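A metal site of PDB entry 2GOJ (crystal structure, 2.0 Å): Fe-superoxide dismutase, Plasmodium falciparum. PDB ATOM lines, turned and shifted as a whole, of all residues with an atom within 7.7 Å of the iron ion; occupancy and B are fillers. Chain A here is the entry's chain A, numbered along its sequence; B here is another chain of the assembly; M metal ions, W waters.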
ATOM      1  N   HIS A  26     -31.997  -6.288  33.359  1.00  0.00           N
ATOM      2  CA  HIS A  26     -31.328  -5.680  32.205  1.00  0.00           C
ATOM      3  C   HIS A  26     -30.737  -6.768  31.284  1.00  0.00           C
ATOM      4  O   HIS A  26     -30.854  -6.681  30.073  1.00  0.00           O
ATOM      5  CB  HIS A  26     -30.233  -4.695  32.694  1.00  0.00           C
ATOM      6  CG  HIS A  26     -29.873  -3.639  31.712  1.00  0.00           C
ATOM      7  ND1 HIS A  26     -29.112  -2.539  32.060  1.00  0.00           N
ATOM      8  CD2 HIS A  26     -30.174  -3.491  30.393  1.00  0.00           C
ATOM      9  CE1 HIS A  26     -28.978  -1.751  30.999  1.00  0.00           C
ATOM     10  NE2 HIS A  26     -29.612  -2.305  29.981  1.00  0.00           N
ATOM     11  N   TYR A  27     -30.142  -7.800  31.874  1.00  0.00           N
ATOM     12  CA  TYR A  27     -29.468  -8.854  31.101  1.00  0.00           C
ATOM     13  C   TYR A  27     -30.414 -10.001  30.739  1.00  0.00           C
ATOM     14  O   TYR A  27     -30.569 -10.320  29.574  1.00  0.00           O
ATOM     15  CB  TYR A  27     -28.274  -9.412  31.871  1.00  0.00           C
ATOM     16  CG  TYR A  27     -27.542 -10.508  31.146  1.00  0.00           C
ATOM     17  CD1 TYR A  27     -26.798 -10.232  29.989  1.00  0.00           C
ATOM     18  CD2 TYR A  27     -27.561 -11.832  31.603  1.00  0.00           C
ATOM     19  CE1 TYR A  27     -26.097 -11.231  29.314  1.00  0.00           C
ATOM     20  CE2 TYR A  27     -26.868 -12.845  30.923  1.00  0.00           C
ATOM     21  CZ  TYR A  27     -26.132 -12.535  29.794  1.00  0.00           C
ATOM     22  OH  TYR A  27     -25.442 -13.521  29.101  1.00  0.00           O
ATOM     23  N   HIS A  30     -34.233  -7.720  29.357  1.00  0.00           N
ATOM     24  CA  HIS A  30     -34.106  -6.790  28.229  1.00  0.00           C
ATOM     25  C   HIS A  30     -33.178  -7.349  27.153  1.00  0.00           C
ATOM     26  O   HIS A  30     -33.558  -7.486  25.985  1.00  0.00           O
ATOM     27  CB  HIS A  30     -33.579  -5.418  28.684  1.00  0.00           C
ATOM     28  CG  HIS A  30     -34.565  -4.628  29.490  1.00  0.00           C
ATOM     29  ND1 HIS A  30     -35.575  -3.888  28.907  1.00  0.00           N
ATOM     30  CD2 HIS A  30     -34.705  -4.489  30.827  1.00  0.00           C
ATOM     31  CE1 HIS A  30     -36.296  -3.320  29.861  1.00  0.00           C
ATOM     32  NE2 HIS A  30     -35.793  -3.657  31.027  1.00  0.00           N
ATOM     33  N   HIS A  31     -31.954  -7.681  27.542  1.00  0.00           N
ATOM     34  CA  HIS A  31     -30.916  -8.063  26.571  1.00  0.00           C
ATOM     35  C   HIS A  31     -31.320  -9.400  25.916  1.00  0.00           C
ATOM     36  O   HIS A  31     -31.248  -9.558  24.689  1.00  0.00           O
ATOM     37  CB  HIS A  31     -29.561  -8.151  27.290  1.00  0.00           C
ATOM     38  CG  HIS A  31     -28.377  -8.181  26.373  1.00  0.00           C
ATOM     39  ND1 HIS A  31     -27.088  -8.284  26.847  1.00  0.00           N
ATOM     40  CD2 HIS A  31     -28.288  -8.151  25.023  1.00  0.00           C
ATOM     41  CE1 HIS A  31     -26.245  -8.314  25.827  1.00  0.00           C
ATOM     42  NE2 HIS A  31     -26.950  -8.228  24.712  1.00  0.00           N
ATOM     43  N   TYR A  34     -34.084  -8.857  23.311  1.00  0.00           N
ATOM     44  CA  TYR A  34     -33.642  -8.384  22.008  1.00  0.00           C
ATOM     45  C   TYR A  34     -33.148  -9.545  21.161  1.00  0.00           C
ATOM     46  O   TYR A  34     -33.394  -9.578  19.964  1.00  0.00           O
ATOM     47  CB  TYR A  34     -32.538  -7.312  22.130  1.00  0.00           C
ATOM     48  CG  TYR A  34     -33.008  -6.009  22.753  1.00  0.00           C
ATOM     49  CD1 TYR A  34     -33.979  -5.235  22.140  1.00  0.00           C
ATOM     50  CD2 TYR A  34     -32.456  -5.556  23.948  1.00  0.00           C
ATOM     51  CE1 TYR A  34     -34.414  -4.045  22.699  1.00  0.00           C
ATOM     52  CE2 TYR A  34     -32.866  -4.345  24.524  1.00  0.00           C
ATOM     53  CZ  TYR A  34     -33.847  -3.608  23.896  1.00  0.00           C
ATOM     54  OH  TYR A  34     -34.263  -2.415  24.441  1.00  0.00           O
ATOM     55  N   GLN A  69     -29.208  -3.094  19.649  1.00  0.00           N
ATOM     56  CA  GLN A  69     -29.384  -3.222  21.093  1.00  0.00           C
ATOM     57  C   GLN A  69     -28.637  -4.424  21.664  1.00  0.00           C
ATOM     58  O   GLN A  69     -28.096  -4.359  22.761  1.00  0.00           O
ATOM     59  CB  GLN A  69     -30.858  -3.265  21.509  1.00  0.00           C
ATOM     60  CG  GLN A  69     -31.574  -1.914  21.469  1.00  0.00           C
ATOM     61  CD  GLN A  69     -31.013  -0.909  22.468  1.00  0.00           C
ATOM     62  OE1 GLN A  69     -29.979  -0.283  22.207  1.00  0.00           O
ATOM     63  NE2 GLN A  69     -31.697  -0.730  23.585  1.00  0.00           N
ATOM     64  N   ASN A  72     -24.979  -3.296  21.466  1.00  0.00           N
ATOM     65  CA  ASN A  72     -24.690  -2.232  22.419  1.00  0.00           C
ATOM     66  C   ASN A  72     -24.700  -2.777  23.840  1.00  0.00           C
ATOM     67  O   ASN A  72     -23.905  -2.324  24.692  1.00  0.00           O
ATOM     68  CB  ASN A  72     -25.723  -1.088  22.349  1.00  0.00           C
ATOM     69  CG  ASN A  72     -25.791  -0.395  20.996  1.00  0.00           C
ATOM     70  OD1 ASN A  72     -24.825  -0.382  20.205  1.00  0.00           O
ATOM     71  ND2 ASN A  72     -26.977   0.153  20.686  1.00  0.00           N
ATOM     72  N   HIS A  73     -25.598  -3.709  24.127  1.00  0.00           N
ATOM     73  CA  HIS A  73     -25.690  -4.264  25.471  1.00  0.00           C
ATOM     74  C   HIS A  73     -24.458  -5.083  25.831  1.00  0.00           C
ATOM     75  O   HIS A  73     -23.929  -4.966  26.932  1.00  0.00           O
ATOM     76  CB  HIS A  73     -26.994  -5.039  25.688  1.00  0.00           C
ATOM     77  CG  HIS A  73     -28.146  -4.135  25.989  1.00  0.00           C
ATOM     78  ND1 HIS A  73     -28.766  -3.388  25.021  1.00  0.00           N
ATOM     79  CD2 HIS A  73     -28.732  -3.793  27.159  1.00  0.00           C
ATOM     80  CE1 HIS A  73     -29.706  -2.641  25.576  1.00  0.00           C
ATOM     81  NE2 HIS A  73     -29.704  -2.868  26.879  1.00  0.00           N
ATOM     82  N   TYR A  76     -21.633  -2.796  26.559  1.00  0.00           N
ATOM     83  CA  TYR A  76     -21.875  -2.205  27.861  1.00  0.00           C
ATOM     84  C   TYR A  76     -21.428  -3.135  29.014  1.00  0.00           C
ATOM     85  O   TYR A  76     -20.734  -2.690  29.925  1.00  0.00           O
ATOM     86  CB  TYR A  76     -23.370  -1.886  27.945  1.00  0.00           C
ATOM     87  CG  TYR A  76     -23.911  -1.425  29.271  1.00  0.00           C
ATOM     88  CD1 TYR A  76     -23.487  -0.241  29.838  1.00  0.00           C
ATOM     89  CD2 TYR A  76     -24.894  -2.165  29.946  1.00  0.00           C
ATOM     90  CE1 TYR A  76     -23.999   0.207  31.046  1.00  0.00           C
ATOM     91  CE2 TYR A  76     -25.401  -1.731  31.164  1.00  0.00           C
ATOM     92  CZ  TYR A  76     -24.964  -0.530  31.708  1.00  0.00           C
ATOM     93  OH  TYR A  76     -25.461  -0.057  32.904  1.00  0.00           O
ATOM     94  N   TRP A  77     -21.795  -4.414  28.953  1.00  0.00           N
ATOM     95  CA  TRP A  77     -21.395  -5.361  30.005  1.00  0.00           C
ATOM     96  C   TRP A  77     -19.876  -5.544  30.029  1.00  0.00           C
ATOM     97  O   TRP A  77     -19.264  -5.584  31.096  1.00  0.00           O
ATOM     98  CB  TRP A  77     -22.071  -6.731  29.838  1.00  0.00           C
ATOM     99  CG  TRP A  77     -23.567  -6.663  29.833  1.00  0.00           C
ATOM    100  CD1 TRP A  77     -24.392  -7.191  28.897  1.00  0.00           C
ATOM    101  CD2 TRP A  77     -24.403  -6.018  30.788  1.00  0.00           C
ATOM    102  NE1 TRP A  77     -25.704  -6.916  29.211  1.00  0.00           N
ATOM    103  CE2 TRP A  77     -25.728  -6.204  30.375  1.00  0.00           C
ATOM    104  CE3 TRP A  77     -24.161  -5.310  31.972  1.00  0.00           C
ATOM    105  CZ2 TRP A  77     -26.819  -5.703  31.092  1.00  0.00           C
ATOM    106  CZ3 TRP A  77     -25.252  -4.818  32.678  1.00  0.00           C
ATOM    107  CH2 TRP A  77     -26.553  -4.999  32.223  1.00  0.00           C
ATOM    108  N   GLY A 121     -31.032   6.191  25.199  1.00  0.00           N
ATOM    109  CA  GLY A 121     -29.810   6.258  24.421  1.00  0.00           C
ATOM    110  C   GLY A 121     -28.552   5.797  25.126  1.00  0.00           C
ATOM    111  O   GLY A 121     -28.591   5.148  26.171  1.00  0.00           O
ATOM    112  N   TRP A 122     -27.413   6.161  24.542  1.00  0.00           N
ATOM    113  CA  TRP A 122     -26.103   5.644  24.909  1.00  0.00           C
ATOM    114  C   TRP A 122     -25.067   6.768  24.903  1.00  0.00           C
ATOM    115  O   TRP A 122     -25.072   7.573  24.000  1.00  0.00           O
ATOM    116  CB  TRP A 122     -25.698   4.547  23.899  1.00  0.00           C
ATOM    117  CG  TRP A 122     -26.657   3.381  23.878  1.00  0.00           C
ATOM    118  CD1 TRP A 122     -27.817   3.291  23.170  1.00  0.00           C
ATOM    119  CD2 TRP A 122     -26.543   2.150  24.615  1.00  0.00           C
ATOM    120  NE1 TRP A 122     -28.440   2.092  23.406  1.00  0.00           N
ATOM    121  CE2 TRP A 122     -27.677   1.367  24.284  1.00  0.00           C
ATOM    122  CE3 TRP A 122     -25.602   1.629  25.499  1.00  0.00           C
ATOM    123  CZ2 TRP A 122     -27.895   0.099  24.828  1.00  0.00           C
ATOM    124  CZ3 TRP A 122     -25.820   0.362  26.043  1.00  0.00           C
ATOM    125  CH2 TRP A 122     -26.956  -0.386  25.711  1.00  0.00           C
ATOM    126  N   ASP A 157     -25.005   2.870  29.113  1.00  0.00           N
ATOM    127  CA  ASP A 157     -26.441   2.866  28.825  1.00  0.00           C
ATOM    128  C   ASP A 157     -27.166   3.876  29.700  1.00  0.00           C
ATOM    129  O   ASP A 157     -27.038   3.845  30.911  1.00  0.00           O
ATOM    130  CB  ASP A 157     -26.961   1.451  29.128  1.00  0.00           C
ATOM    131  CG  ASP A 157     -28.345   1.179  28.579  1.00  0.00           C
ATOM    132  OD1 ASP A 157     -29.018   2.101  28.063  1.00  0.00           O
ATOM    133  OD2 ASP A 157     -28.846   0.020  28.640  1.00  0.00           O
ATOM    134  N   ILE A 158     -27.953   4.752  29.084  1.00  0.00           N
ATOM    135  CA  ILE A 158     -28.771   5.698  29.845  1.00  0.00           C
ATOM    136  C   ILE A 158     -30.284   5.610  29.520  1.00  0.00           C
ATOM    137  O   ILE A 158     -31.067   6.494  29.857  1.00  0.00           O
ATOM    138  CB  ILE A 158     -28.215   7.148  29.748  1.00  0.00           C
ATOM    139  CG1 ILE A 158     -28.034   7.598  28.300  1.00  0.00           C
ATOM    140  CG2 ILE A 158     -26.872   7.271  30.472  1.00  0.00           C
ATOM    141  CD1 ILE A 158     -29.235   8.127  27.708  1.00  0.00           C
ATOM    142  N   TRP A 159     -30.708   4.524  28.884  1.00  0.00           N
ATOM    143  CA  TRP A 159     -32.115   4.133  28.911  1.00  0.00           C
ATOM    144  C   TRP A 159     -32.495   4.053  30.385  1.00  0.00           C
ATOM    145  O   TRP A 159     -31.694   3.625  31.214  1.00  0.00           O
ATOM    146  CB  TRP A 159     -32.326   2.758  28.282  1.00  0.00           C
ATOM    147  CG  TRP A 159     -32.303   2.692  26.777  1.00  0.00           C
ATOM    148  CD1 TRP A 159     -31.242   2.992  25.959  1.00  0.00           C
ATOM    149  CD2 TRP A 159     -33.362   2.268  25.937  1.00  0.00           C
ATOM    150  NE1 TRP A 159     -31.604   2.782  24.649  1.00  0.00           N
ATOM    151  CE2 TRP A 159     -32.905   2.333  24.606  1.00  0.00           C
ATOM    152  CE3 TRP A 159     -34.678   1.826  26.162  1.00  0.00           C
ATOM    153  CZ2 TRP A 159     -33.696   1.993  23.510  1.00  0.00           C
ATOM    154  CZ3 TRP A 159     -35.481   1.488  25.074  1.00  0.00           C
ATOM    155  CH2 TRP A 159     -34.981   1.573  23.760  1.00  0.00           C
ATOM    156  N   GLU A 160     -33.712   4.452  30.722  1.00  0.00           N
ATOM    157  CA  GLU A 160     -34.150   4.469  32.131  1.00  0.00           C
ATOM    158  C   GLU A 160     -34.055   3.114  32.841  1.00  0.00           C
ATOM    159  O   GLU A 160     -33.764   3.082  34.023  1.00  0.00           O
ATOM    160  CB  GLU A 160     -35.550   5.086  32.261  1.00  0.00           C
ATOM    161  CG  GLU A 160     -35.576   6.538  31.813  1.00  0.00           C
ATOM    162  CD  GLU A 160     -36.955   7.175  31.853  1.00  0.00           C
ATOM    163  OE1 GLU A 160     -37.947   6.560  31.360  1.00  0.00           O
ATOM    164  OE2 GLU A 160     -37.026   8.338  32.353  1.00  0.00           O
ATOM    165  N   HIS A 161     -34.241   2.018  32.125  1.00  0.00           N
ATOM    166  CA  HIS A 161     -34.160   0.673  32.709  1.00  0.00           C
ATOM    167  C   HIS A 161     -32.771   0.326  33.253  1.00  0.00           C
ATOM    168  O   HIS A 161     -32.648  -0.528  34.114  1.00  0.00           O
ATOM    169  CB  HIS A 161     -34.642  -0.410  31.722  1.00  0.00           C
ATOM    170  CG  HIS A 161     -33.791  -0.559  30.497  1.00  0.00           C
ATOM    171  ND1 HIS A 161     -34.303  -0.432  29.219  1.00  0.00           N
ATOM    172  CD2 HIS A 161     -32.475  -0.876  30.343  1.00  0.00           C
ATOM    173  CE1 HIS A 161     -33.337  -0.656  28.336  1.00  0.00           C
ATOM    174  NE2 HIS A 161     -32.219  -0.906  29.001  1.00  0.00           N
ATOM    175  N   ALA A 162     -31.744   1.017  32.759  1.00  0.00           N
ATOM    176  CA  ALA A 162     -30.379   0.813  33.236  1.00  0.00           C
ATOM    177  C   ALA A 162     -30.207   1.233  34.700  1.00  0.00           C
ATOM    178  O   ALA A 162     -29.334   0.698  35.400  1.00  0.00           O
ATOM    179  CB  ALA A 162     -29.411   1.548  32.376  1.00  0.00           C
ATOM    180  N   TYR A 174     -26.412   7.429  39.165  1.00  0.00           N
ATOM    181  CA  TYR A 174     -26.102   6.233  38.377  1.00  0.00           C
ATOM    182  C   TYR A 174     -24.763   6.433  37.664  1.00  0.00           C
ATOM    183  O   TYR A 174     -23.908   5.570  37.704  1.00  0.00           O
ATOM    184  CB  TYR A 174     -27.195   5.956  37.341  1.00  0.00           C
ATOM    185  CG  TYR A 174     -26.790   5.054  36.194  1.00  0.00           C
ATOM    186  CD1 TYR A 174     -26.471   3.707  36.403  1.00  0.00           C
ATOM    187  CD2 TYR A 174     -26.788   5.540  34.894  1.00  0.00           C
ATOM    188  CE1 TYR A 174     -26.130   2.874  35.332  1.00  0.00           C
ATOM    189  CE2 TYR A 174     -26.445   4.721  33.821  1.00  0.00           C
ATOM    190  CZ  TYR A 174     -26.112   3.402  34.042  1.00  0.00           C
ATOM    191  OH  TYR A 174     -25.772   2.614  32.981  1.00  0.00           O
ATOM    192  N   GLU B 160     -40.174   4.575  30.015  1.00  0.00           N
ATOM    193  CA  GLU B 160     -40.005   3.512  30.995  1.00  0.00           C
ATOM    194  C   GLU B 160     -40.293   3.969  32.424  1.00  0.00           C
ATOM    195  O   GLU B 160     -40.784   3.171  33.211  1.00  0.00           O
ATOM    196  CB  GLU B 160     -38.632   2.863  30.874  1.00  0.00           C
ATOM    197  CG  GLU B 160     -38.399   2.121  29.567  1.00  0.00           C
ATOM    198  CD  GLU B 160     -37.002   1.535  29.449  1.00  0.00           C
ATOM    199  OE1 GLU B 160     -36.011   2.224  29.765  1.00  0.00           O
ATOM    200  OE2 GLU B 160     -36.898   0.370  29.011  1.00  0.00           O
HETATM  201 FE    FE M   1     -30.306  -1.170  28.202  1.00  0.00          FE
HETATM  202  O   HOH W   1     -30.805  -0.032  26.580  1.00  0.00           O
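The side-chain hydroxyl (OH) of Tyr 174 lies within hydrogen-bond range of the backbone carbonyl oxygen (O) of Asp 157, 2.7 Å away. The backbone NH (N) of Trp 159 lies within hydrogen-bond range of the side-chain carboxylate (OD1) of Asp 157, 3.1 Å away. The indole nitrogen (NE1) of Trp 77 sits close to the backbone carbonyl oxygen (O) of His 73, at 3.5 Å. The side-chain carboxylate of Glu 160 of chain B sits at hydrogen-bond distance from a ring nitrogen (ND1) of His 161. The backbone NH of His 31 lies within hydrogen-bond range of the backbone carbonyl oxygen of His 26, at 2.9 Å. ND1 of His 73 lies within hydrogen-bond range of O of Gln 69 (2.5 Å).
Four residues have an atom within 4 Å of the iron ion: His 26, His 73, Asp 157 and His 161. Along chain A the residues within 4 Å of the iron ion span positions 26 to 161.
The iron ion is bound by OD2 of Asp 157 (1.9 Å), water W1 (2.0 Å), NE2 of His 161 (2.1 Å), NE2 of His 26 (2.2 Å) and NE2 of His 73 (2.2 Å). The iron ion has five donor atoms within binding distance.
Water W1 bridges OD1 of Asp 157 and NE2 of Gln 69.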
